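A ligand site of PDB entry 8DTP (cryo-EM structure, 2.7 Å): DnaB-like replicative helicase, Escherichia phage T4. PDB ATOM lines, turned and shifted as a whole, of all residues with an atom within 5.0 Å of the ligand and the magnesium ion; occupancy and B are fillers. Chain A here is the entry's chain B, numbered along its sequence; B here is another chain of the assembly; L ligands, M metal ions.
The side-chain amino group (NZ) of Lys 203 is in hydrogen-bond range of an oxygen (O1) of the ligand, at 3.2 Å.
The backbone NH (N) of Leu 205 is in hydrogen-bond range of an oxygen (O6) of the ligand (2.9 Å).
N3 of the ligand sits at hydrogen-bond distance from O of Tyr 408 of chain B, 3.2 Å away.
An oxygen (O4) of the ligand is in salt-bridge range of the side-chain amino group of Lys 405 of chain B, 3.9 Å away.
The backbone carbonyl oxygen of Gly 202 sits close to an oxygen (O8) of the ligand (2.7 Å).
The backbone NH (N) of Asn 200 lies close to a sulfur (S1) of the ligand (2.9 Å).
NE of Arg 407 of chain B is in hydrogen-bond range of O2 of the ligand (3.4 Å).
An oxygen (O6) of the ligand is in salt-bridge range of the guanidinium group (NH2) of Arg 236.
NZ of Lys 423 sits close to O11 of the ligand (3.2 Å).
OD1 of Asp 410 of chain B sits at hydrogen-bond distance from O12 of the ligand (3.4 Å).
OD1 of Asn 200 lies close to O4 of the ligand (2.8 Å).
The side-chain carboxylate of Asp 247 sits close to a nitrogen (N4) of the ligand, at 3.4 Å.
CA of Val 199 touches S1 of the ligand, 3.6 Å away.
Val 201 touches the ligand.
Leu 246 touches the ligand (CD2 to N3, 3.4 Å).
Gln 426 touches the ligand (NE2 to N1, 3.6 Å).
O of Ala 379 of chain B touches O1 of the ligand, at 3.9 Å.
Gly 409 of chain B touches the ligand (CA to N3, 3.98 Å).
Hydrophobic or aromatic side chains that line the ligand: Val 199, Leu 205 and Leu 246.
The nearest printed residue that does not touch the ligand is Tyr 312 (4.3 Å).
Lys 203 touches the magnesium ion (NZ to MG, 3.7 Å).
Of the 27 residues printed, 3 come within 4 Å of the magnesium ion.
Along chain A the residues within 4 Å of the magnesium ion span positions 203 to 227.
The backbone carbonyl oxygen of Glu 227 sits at hydrogen-bond distance from the guanidinium group of Arg 407 of chain B (2.9 Å).
The side-chain carboxylate (OE2) of Glu 227 lies close to the side-chain hydroxyl (OG) of Ser 204, 3.1 Å away.
NZ of Lys 405 of chain B is in hydrogen-bond range of OD1 of Asn 200 (2.6 Å).
OD1 of Asp 311 is in hydrogen-bond range of OG of Ser 204, 2.6 Å away.
The guanidinium group of Arg 236 is in hydrogen-bond range of the side-chain sulfur of Met 228.
The side-chain amide nitrogen (NE2) of Gln 426 lies within hydrogen-bond range of the backbone carbonyl oxygen (O) of Lys 423, at 3.1 Å.
ND2 of Asn 200 lies close to NZ of Lys 411 of chain B (3.0 Å).
The guanidinium group (NH2) of Arg 236 is in hydrogen-bond range of the side-chain amide oxygen (OE1) of Gln 426, 2.6 Å away.
The magnesium ion is bound by an oxygen (O5) of the ligand (2.0 Å), the side-chain carboxylate (OE2) of Glu 227 (2.0 Å) and an oxygen (O8) of the ligand (2.5 Å).
The magnesium ion has three donor atoms within binding distance.
Slightly farther from the magnesium ion lies OG of Ser 204 (2.8 Å).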
ATOM      1  N   GLY A 198       3.834 -19.710   5.919  1.00  0.00           N
ATOM      2  CA  GLY A 198       3.280 -20.816   5.147  1.00  0.00           C
ATOM      3  C   GLY A 198       3.889 -20.864   3.757  1.00  0.00           C
ATOM      4  O   GLY A 198       5.070 -20.577   3.567  1.00  0.00           O
ATOM      5  N   VAL A 199       3.058 -21.242   2.785  1.00  0.00           N
ATOM      6  CA  VAL A 199       3.471 -21.364   1.390  1.00  0.00           C
ATOM      7  C   VAL A 199       2.758 -20.289   0.588  1.00  0.00           C
ATOM      8  O   VAL A 199       1.523 -20.265   0.534  1.00  0.00           O
ATOM      9  CB  VAL A 199       3.180 -22.757   0.833  1.00  0.00           C
ATOM     10  CG1 VAL A 199       3.437 -22.799  -0.657  1.00  0.00           C
ATOM     11  CG2 VAL A 199       4.011 -23.801   1.553  1.00  0.00           C
ATOM     12  N   ASN A 200       3.535 -19.424  -0.059  1.00  0.00           N
ATOM     13  CA  ASN A 200       3.009 -18.311  -0.844  1.00  0.00           C
ATOM     14  C   ASN A 200       2.028 -17.461  -0.037  1.00  0.00           C
ATOM     15  O   ASN A 200       0.992 -17.018  -0.529  1.00  0.00           O
ATOM     16  CB  ASN A 200       2.348 -18.807  -2.138  1.00  0.00           C
ATOM     17  CG  ASN A 200       3.337 -18.974  -3.277  1.00  0.00           C
ATOM     18  OD1 ASN A 200       4.550 -18.978  -3.063  1.00  0.00           O
ATOM     19  ND2 ASN A 200       2.830 -19.126  -4.487  1.00  0.00           N
ATOM     20  N   VAL A 201       2.369 -17.240   1.229  1.00  0.00           N
ATOM     21  CA  VAL A 201       1.597 -16.369   2.101  1.00  0.00           C
ATOM     22  C   VAL A 201       2.317 -15.058   2.386  1.00  0.00           C
ATOM     23  O   VAL A 201       1.658 -14.066   2.728  1.00  0.00           O
ATOM     24  CB  VAL A 201       1.238 -17.071   3.423  1.00  0.00           C
ATOM     25  CG1 VAL A 201       0.116 -16.342   4.142  1.00  0.00           C
ATOM     26  CG2 VAL A 201       0.849 -18.519   3.161  1.00  0.00           C
ATOM     27  N   GLY A 202       3.637 -15.000   2.225  1.00  0.00           N
ATOM     28  CA  GLY A 202       4.452 -13.884   2.661  1.00  0.00           C
ATOM     29  C   GLY A 202       5.865 -14.384   2.840  1.00  0.00           C
ATOM     30  O   GLY A 202       6.442 -14.943   1.901  1.00  0.00           O
ATOM     31  N   LYS A 203       6.464 -14.127   3.996  1.00  0.00           N
ATOM     32  CA  LYS A 203       7.671 -14.834   4.431  1.00  0.00           C
ATOM     33  C   LYS A 203       8.893 -14.390   3.616  1.00  0.00           C
ATOM     34  O   LYS A 203      10.033 -14.750   3.930  1.00  0.00           O
ATOM     35  CB  LYS A 203       7.458 -16.340   4.327  1.00  0.00           C
ATOM     36  CG  LYS A 203       8.384 -17.192   5.150  1.00  0.00           C
ATOM     37  CD  LYS A 203       8.017 -18.660   5.043  1.00  0.00           C
ATOM     38  CE  LYS A 203       8.006 -19.119   3.595  1.00  0.00           C
ATOM     39  NZ  LYS A 203       9.315 -18.903   2.924  1.00  0.00           N
ATOM     40  N   SER A 204       8.644 -13.612   2.573  1.00  0.00           N
ATOM     41  CA  SER A 204       9.670 -12.855   1.863  1.00  0.00           C
ATOM     42  C   SER A 204       9.182 -11.467   1.460  1.00  0.00           C
ATOM     43  O   SER A 204      10.016 -10.575   1.291  1.00  0.00           O
ATOM     44  CB  SER A 204      10.143 -13.609   0.613  1.00  0.00           C
ATOM     45  OG  SER A 204      10.931 -14.725   0.958  1.00  0.00           O
ATOM     46  N   LEU A 205       7.873 -11.274   1.296  1.00  0.00           N
ATOM     47  CA  LEU A 205       7.309  -9.940   1.261  1.00  0.00           C
ATOM     48  C   LEU A 205       7.570  -9.211   2.578  1.00  0.00           C
ATOM     49  O   LEU A 205       7.940  -8.033   2.594  1.00  0.00           O
ATOM     50  CB  LEU A 205       5.811 -10.015   0.970  1.00  0.00           C
ATOM     51  CG  LEU A 205       4.993  -8.775   0.567  1.00  0.00           C
ATOM     52  CD1 LEU A 205       3.694  -9.212  -0.094  1.00  0.00           C
ATOM     53  CD2 LEU A 205       4.689  -7.862   1.748  1.00  0.00           C
ATOM     54  N   GLU A 227      16.660 -18.803  -1.739  1.00  0.00           N
ATOM     55  CA  GLU A 227      15.606 -19.284  -2.625  1.00  0.00           C
ATOM     56  C   GLU A 227      15.349 -18.384  -3.827  1.00  0.00           C
ATOM     57  O   GLU A 227      14.682 -18.815  -4.759  1.00  0.00           O
ATOM     58  CB  GLU A 227      14.294 -19.453  -1.847  1.00  0.00           C
ATOM     59  CG  GLU A 227      13.669 -18.137  -1.405  1.00  0.00           C
ATOM     60  CD  GLU A 227      12.328 -18.328  -0.739  1.00  0.00           C
ATOM     61  OE1 GLU A 227      11.966 -19.483  -0.435  1.00  0.00           O
ATOM     62  OE2 GLU A 227      11.617 -17.319  -0.516  1.00  0.00           O
ATOM     63  N   MET A 228      15.855 -17.154  -3.819  1.00  0.00           N
ATOM     64  CA  MET A 228      15.645 -16.224  -4.917  1.00  0.00           C
ATOM     65  C   MET A 228      16.961 -15.600  -5.332  1.00  0.00           C
ATOM     66  O   MET A 228      17.881 -15.454  -4.524  1.00  0.00           O
ATOM     67  CB  MET A 228      14.645 -15.115  -4.538  1.00  0.00           C
ATOM     68  CG  MET A 228      13.206 -15.580  -4.420  1.00  0.00           C
ATOM     69  SD  MET A 228      12.067 -14.227  -4.109  1.00  0.00           S
ATOM     70  CE  MET A 228      12.669 -13.632  -2.525  1.00  0.00           C
ATOM     71  N   ARG A 236      11.948  -6.693  -5.870  1.00  0.00           N
ATOM     72  CA  ARG A 236      10.949  -6.528  -4.816  1.00  0.00           C
ATOM     73  C   ARG A 236      11.243  -5.293  -3.979  1.00  0.00           C
ATOM     74  O   ARG A 236      10.331  -4.538  -3.606  1.00  0.00           O
ATOM     75  CB  ARG A 236      10.895  -7.785  -3.943  1.00  0.00           C
ATOM     76  CG  ARG A 236      10.714  -9.054  -4.737  1.00  0.00           C
ATOM     77  CD  ARG A 236      10.536 -10.277  -3.857  1.00  0.00           C
ATOM     78  NE  ARG A 236       9.130 -10.522  -3.577  1.00  0.00           N
ATOM     79  CZ  ARG A 236       8.638 -11.683  -3.174  1.00  0.00           C
ATOM     80  NH1 ARG A 236       9.421 -12.733  -2.978  1.00  0.00           N
ATOM     81  NH2 ARG A 236       7.332 -11.794  -2.952  1.00  0.00           N
ATOM     82  N   LEU A 246       4.811  -4.469  -8.833  1.00  0.00           N
ATOM     83  CA  LEU A 246       5.772  -5.471  -9.282  1.00  0.00           C
ATOM     84  C   LEU A 246       5.461  -5.940 -10.697  1.00  0.00           C
ATOM     85  O   LEU A 246       6.376  -6.341 -11.422  1.00  0.00           O
ATOM     86  CB  LEU A 246       5.782  -6.656  -8.313  1.00  0.00           C
ATOM     87  CG  LEU A 246       7.024  -7.533  -8.314  1.00  0.00           C
ATOM     88  CD1 LEU A 246       8.262  -6.699  -8.056  1.00  0.00           C
ATOM     89  CD2 LEU A 246       6.896  -8.638  -7.282  1.00  0.00           C
ATOM     90  N   ASP A 247       4.195  -5.895 -11.100  1.00  0.00           N
ATOM     91  CA  ASP A 247       3.845  -6.260 -12.477  1.00  0.00           C
ATOM     92  C   ASP A 247       4.253  -5.151 -13.447  1.00  0.00           C
ATOM     93  O   ASP A 247       4.639  -5.438 -14.590  1.00  0.00           O
ATOM     94  CB  ASP A 247       2.353  -6.552 -12.578  1.00  0.00           C
ATOM     95  CG  ASP A 247       1.933  -7.754 -11.757  1.00  0.00           C
ATOM     96  OD1 ASP A 247       2.757  -8.680 -11.611  1.00  0.00           O
ATOM     97  OD2 ASP A 247       0.790  -7.774 -11.262  1.00  0.00           O
ATOM     98  N   ASP A 250       7.560  -5.464 -14.903  1.00  0.00           N
ATOM     99  CA  ASP A 250       7.691  -6.600 -15.817  1.00  0.00           C
ATOM    100  C   ASP A 250       7.041  -6.335 -17.169  1.00  0.00           C
ATOM    101  O   ASP A 250       7.663  -6.563 -18.210  1.00  0.00           O
ATOM    102  CB  ASP A 250       7.085  -7.858 -15.182  1.00  0.00           C
ATOM    103  CG  ASP A 250       7.850  -8.318 -13.958  1.00  0.00           C
ATOM    104  OD1 ASP A 250       9.075  -8.082 -13.894  1.00  0.00           O
ATOM    105  OD2 ASP A 250       7.222  -8.909 -13.056  1.00  0.00           O
ATOM    106  N   ASP A 311      16.929 -15.204   3.931  1.00  0.00           N
ATOM    107  CA  ASP A 311      15.611 -15.396   3.319  1.00  0.00           C
ATOM    108  C   ASP A 311      14.916 -16.655   3.823  1.00  0.00           C
ATOM    109  O   ASP A 311      13.688 -16.728   3.787  1.00  0.00           O
ATOM    110  CB  ASP A 311      15.740 -15.454   1.801  1.00  0.00           C
ATOM    111  CG  ASP A 311      14.435 -15.164   1.095  1.00  0.00           C
ATOM    112  OD1 ASP A 311      13.445 -14.836   1.774  1.00  0.00           O
ATOM    113  OD2 ASP A 311      14.404 -15.250  -0.155  1.00  0.00           O
ATOM    114  N   TYR A 312      15.673 -17.640   4.309  1.00  0.00           N
ATOM    115  CA  TYR A 312      15.078 -18.902   4.757  1.00  0.00           C
ATOM    116  C   TYR A 312      16.074 -19.614   5.650  1.00  0.00           C
ATOM    117  O   TYR A 312      17.191 -19.903   5.210  1.00  0.00           O
ATOM    118  CB  TYR A 312      14.696 -19.756   3.554  1.00  0.00           C
ATOM    119  CG  TYR A 312      13.600 -20.767   3.813  1.00  0.00           C
ATOM    120  CD1 TYR A 312      13.883 -21.972   4.438  1.00  0.00           C
ATOM    121  CD2 TYR A 312      12.299 -20.532   3.397  1.00  0.00           C
ATOM    122  CE1 TYR A 312      12.892 -22.907   4.670  1.00  0.00           C
ATOM    123  CE2 TYR A 312      11.307 -21.456   3.613  1.00  0.00           C
ATOM    124  CZ  TYR A 312      11.598 -22.644   4.249  1.00  0.00           C
ATOM    125  OH  TYR A 312      10.617 -23.573   4.473  1.00  0.00           O
ATOM    126  N   GLN A 355       9.025 -22.167   7.994  1.00  0.00           N
ATOM    127  CA  GLN A 355       7.825 -22.710   7.304  1.00  0.00           C
ATOM    128  C   GLN A 355       6.844 -23.275   8.339  1.00  0.00           C
ATOM    129  O   GLN A 355       7.286 -23.958   9.268  1.00  0.00           O
ATOM    130  CB  GLN A 355       8.262 -23.788   6.306  1.00  0.00           C
ATOM    131  CG  GLN A 355       7.269 -24.012   5.181  1.00  0.00           C
ATOM    132  CD  GLN A 355       7.499 -23.056   4.041  1.00  0.00           C
ATOM    133  OE1 GLN A 355       8.429 -22.255   4.048  1.00  0.00           O
ATOM    134  NE2 GLN A 355       6.634 -23.125   3.040  1.00  0.00           N
ATOM    135  N   LYS A 423       0.576  -6.721  -1.839  1.00  0.00           N
ATOM    136  CA  LYS A 423       1.414  -7.673  -2.552  1.00  0.00           C
ATOM    137  C   LYS A 423       1.945  -7.114  -3.859  1.00  0.00           C
ATOM    138  O   LYS A 423       3.031  -7.514  -4.301  1.00  0.00           O
ATOM    139  CB  LYS A 423       0.622  -8.963  -2.806  1.00  0.00           C
ATOM    140  CG  LYS A 423       0.150  -9.640  -1.534  1.00  0.00           C
ATOM    141  CD  LYS A 423      -0.644 -10.895  -1.837  1.00  0.00           C
ATOM    142  CE  LYS A 423      -1.096 -11.576  -0.557  1.00  0.00           C
ATOM    143  NZ  LYS A 423      -1.861 -12.819  -0.840  1.00  0.00           N
ATOM    144  N   GLN A 426       4.614  -5.097  -2.628  1.00  0.00           N
ATOM    145  CA  GLN A 426       5.429  -5.932  -1.738  1.00  0.00           C
ATOM    146  C   GLN A 426       5.810  -5.181  -0.473  1.00  0.00           C
ATOM    147  O   GLN A 426       6.999  -5.011  -0.161  1.00  0.00           O
ATOM    148  CB  GLN A 426       6.675  -6.451  -2.464  1.00  0.00           C
ATOM    149  CG  GLN A 426       6.381  -7.405  -3.619  1.00  0.00           C
ATOM    150  CD  GLN A 426       6.240  -8.837  -3.153  1.00  0.00           C
ATOM    151  OE1 GLN A 426       6.945  -9.288  -2.248  1.00  0.00           O
ATOM    152  NE2 GLN A 426       5.336  -9.570  -3.783  1.00  0.00           N
ATOM    153  N   PRO B 378       6.282 -27.735  -2.484  1.00  0.00           N
ATOM    154  CA  PRO B 378       5.872 -26.322  -2.509  1.00  0.00           C
ATOM    155  C   PRO B 378       6.646 -25.476  -1.515  1.00  0.00           C
ATOM    156  O   PRO B 378       6.077 -24.622  -0.823  1.00  0.00           O
ATOM    157  CB  PRO B 378       4.381 -26.375  -2.165  1.00  0.00           C
ATOM    158  CG  PRO B 378       3.990 -27.806  -2.257  1.00  0.00           C
ATOM    159  CD  PRO B 378       5.213 -28.582  -1.932  1.00  0.00           C
ATOM    160  N   ALA B 379       7.948 -25.713  -1.429  1.00  0.00           N
ATOM    161  CA  ALA B 379       8.872 -24.841  -0.716  1.00  0.00           C
ATOM    162  C   ALA B 379      10.180 -24.615  -1.454  1.00  0.00           C
ATOM    163  O   ALA B 379      10.843 -23.602  -1.203  1.00  0.00           O
ATOM    164  CB  ALA B 379       9.184 -25.414   0.672  1.00  0.00           C
ATOM    165  N   LYS B 405       1.665 -23.280  -7.528  1.00  0.00           N
ATOM    166  CA  LYS B 405       2.667 -22.376  -6.906  1.00  0.00           C
ATOM    167  C   LYS B 405       3.444 -21.628  -7.999  1.00  0.00           C
ATOM    168  O   LYS B 405       4.049 -22.298  -8.845  1.00  0.00           O
ATOM    169  CB  LYS B 405       3.676 -23.128  -6.042  1.00  0.00           C
ATOM    170  CG  LYS B 405       4.833 -22.288  -5.521  1.00  0.00           C
ATOM    171  CD  LYS B 405       5.752 -23.042  -4.593  1.00  0.00           C
ATOM    172  CE  LYS B 405       6.796 -22.160  -3.952  1.00  0.00           C
ATOM    173  NZ  LYS B 405       6.186 -21.044  -3.187  1.00  0.00           N
ATOM    174  N   ARG B 407       6.174 -18.678  -8.193  1.00  0.00           N
ATOM    175  CA  ARG B 407       7.084 -17.626  -7.672  1.00  0.00           C
ATOM    176  C   ARG B 407       7.172 -16.529  -8.731  1.00  0.00           C
ATOM    177  O   ARG B 407       7.249 -15.344  -8.355  1.00  0.00           O
ATOM    178  CB  ARG B 407       8.454 -18.234  -7.359  1.00  0.00           C
ATOM    179  CG  ARG B 407       9.273 -17.437  -6.340  1.00  0.00           C
ATOM    180  CD  ARG B 407      10.447 -18.240  -5.824  1.00  0.00           C
ATOM    181  NE  ARG B 407      10.034 -19.523  -5.253  1.00  0.00           N
ATOM    182  CZ  ARG B 407      10.854 -20.415  -4.719  1.00  0.00           C
ATOM    183  NH1 ARG B 407      12.135 -20.123  -4.571  1.00  0.00           N
ATOM    184  NH2 ARG B 407      10.393 -21.593  -4.341  1.00  0.00           N
ATOM    185  N   TYR B 408       7.144 -16.909 -10.014  1.00  0.00           N
ATOM    186  CA  TYR B 408       7.232 -15.937 -11.123  1.00  0.00           C
ATOM    187  C   TYR B 408       6.163 -14.840 -10.980  1.00  0.00           C
ATOM    188  O   TYR B 408       6.553 -13.660 -10.878  1.00  0.00           O
ATOM    189  CB  TYR B 408       7.089 -16.647 -12.470  1.00  0.00           C
ATOM    190  CG  TYR B 408       8.117 -17.732 -12.724  1.00  0.00           C
ATOM    191  CD1 TYR B 408       9.469 -17.446 -12.718  1.00  0.00           C
ATOM    192  CD2 TYR B 408       7.738 -19.042 -12.953  1.00  0.00           C
ATOM    193  CE1 TYR B 408      10.418 -18.428 -12.934  1.00  0.00           C
ATOM    194  CE2 TYR B 408       8.668 -20.035 -13.175  1.00  0.00           C
ATOM    195  CZ  TYR B 408      10.018 -19.729 -13.179  1.00  0.00           C
ATOM    196  OH  TYR B 408      10.947 -20.699 -13.398  1.00  0.00           O
ATOM    197  N   GLY B 409       4.878 -15.212 -10.976  1.00  0.00           N
ATOM    198  CA  GLY B 409       3.824 -14.173 -10.959  1.00  0.00           C
ATOM    199  C   GLY B 409       2.706 -14.522  -9.987  1.00  0.00           C
ATOM    200  O   GLY B 409       2.878 -15.471  -9.216  1.00  0.00           O
ATOM    201  N   ASP B 410       1.604 -13.764 -10.027  1.00  0.00           N
ATOM    202  CA  ASP B 410       0.481 -14.051  -9.146  1.00  0.00           C
ATOM    203  C   ASP B 410      -0.126 -15.396  -9.509  1.00  0.00           C
ATOM    204  O   ASP B 410      -0.412 -15.682 -10.676  1.00  0.00           O
ATOM    205  CB  ASP B 410      -0.568 -12.948  -9.255  1.00  0.00           C
ATOM    206  CG  ASP B 410      -1.598 -13.020  -8.145  1.00  0.00           C
ATOM    207  OD1 ASP B 410      -1.445 -13.859  -7.236  1.00  0.00           O
ATOM    208  OD2 ASP B 410      -2.571 -12.238  -8.187  1.00  0.00           O
ATOM    209  N   LYS B 411      -0.324 -16.242  -8.489  1.00  0.00           N
ATOM    210  CA  LYS B 411      -0.840 -17.589  -8.735  1.00  0.00           C
ATOM    211  C   LYS B 411      -2.295 -17.566  -9.180  1.00  0.00           C
ATOM    212  O   LYS B 411      -2.726 -18.457  -9.932  1.00  0.00           O
ATOM    213  CB  LYS B 411      -0.698 -18.426  -7.460  1.00  0.00           C
ATOM    214  CG  LYS B 411      -1.096 -19.882  -7.606  1.00  0.00           C
ATOM    215  CD  LYS B 411      -1.875 -20.354  -6.383  1.00  0.00           C
ATOM    216  CE  LYS B 411      -1.175 -19.971  -5.097  1.00  0.00           C
ATOM    217  NZ  LYS B 411       0.194 -20.554  -4.998  1.00  0.00           N
HETATM  218  P1  LIG L   1       8.072 -19.579  -0.654  1.00  0.00           P
HETATM  219  S1  LIG L   1       6.225 -20.216  -0.598  1.00  0.00           S
HETATM  220  O1  LIG L   1       8.976 -20.525   0.179  1.00  0.00           O
HETATM  221  O2  LIG L   1       8.565 -19.551  -2.132  1.00  0.00           O
HETATM  222  P2  LIG L   1       7.007 -17.106  -0.436  1.00  0.00           P
HETATM  223  O3  LIG L   1       5.878 -17.191   0.524  1.00  0.00           O
HETATM  224  O4  LIG L   1       6.583 -17.416  -1.882  1.00  0.00           O
HETATM  225  O5  LIG L   1       8.139 -18.134  -0.074  1.00  0.00           O
HETATM  226  P3  LIG L   1       6.917 -14.504  -1.311  1.00  0.00           P
HETATM  227  O6  LIG L   1       7.213 -13.173  -0.735  1.00  0.00           O
HETATM  228  O7  LIG L   1       7.366 -14.691  -2.765  1.00  0.00           O
HETATM  229  O8  LIG L   1       7.616 -15.647  -0.482  1.00  0.00           O
HETATM  230  O9  LIG L   1       5.371 -14.747  -1.156  1.00  0.00           O
HETATM  231  C1  LIG L   1       4.510 -14.871  -2.305  1.00  0.00           C
HETATM  232  C2  LIG L   1       3.407 -13.837  -2.215  1.00  0.00           C
HETATM  233  O10 LIG L   1       3.761 -12.694  -3.013  1.00  0.00           O
HETATM  234  C3  LIG L   1       2.050 -14.304  -2.735  1.00  0.00           C
HETATM  235  O11 LIG L   1       0.994 -13.641  -2.053  1.00  0.00           O
HETATM  236  C4  LIG L   1       2.123 -13.905  -4.215  1.00  0.00           C
HETATM  237  O12 LIG L   1       0.821 -13.662  -4.747  1.00  0.00           O
HETATM  238  C5  LIG L   1       2.936 -12.621  -4.161  1.00  0.00           C
HETATM  239  N1  LIG L   1       3.794 -12.406  -5.321  1.00  0.00           N
HETATM  240  C6  LIG L   1       5.013 -12.983  -5.564  1.00  0.00           C
HETATM  241  N2  LIG L   1       5.558 -12.606  -6.694  1.00  0.00           N
HETATM  242  C7  LIG L   1       4.639 -11.725  -7.242  1.00  0.00           C
HETATM  243  C8  LIG L   1       4.624 -10.984  -8.433  1.00  0.00           C
HETATM  244  N3  LIG L   1       5.611 -11.008  -9.339  1.00  0.00           N
HETATM  245  N4  LIG L   1       3.550 -10.195  -8.672  1.00  0.00           N
HETATM  246  C9  LIG L   1       2.563 -10.165  -7.774  1.00  0.00           C
HETATM  247  N5  LIG L   1       2.461 -10.828  -6.621  1.00  0.00           N
HETATM  248  C10 LIG L   1       3.544 -11.599  -6.406  1.00  0.00           C
HETATM  249 MG    MG M   1       9.702 -16.945  -0.184  1.00  0.00          MG
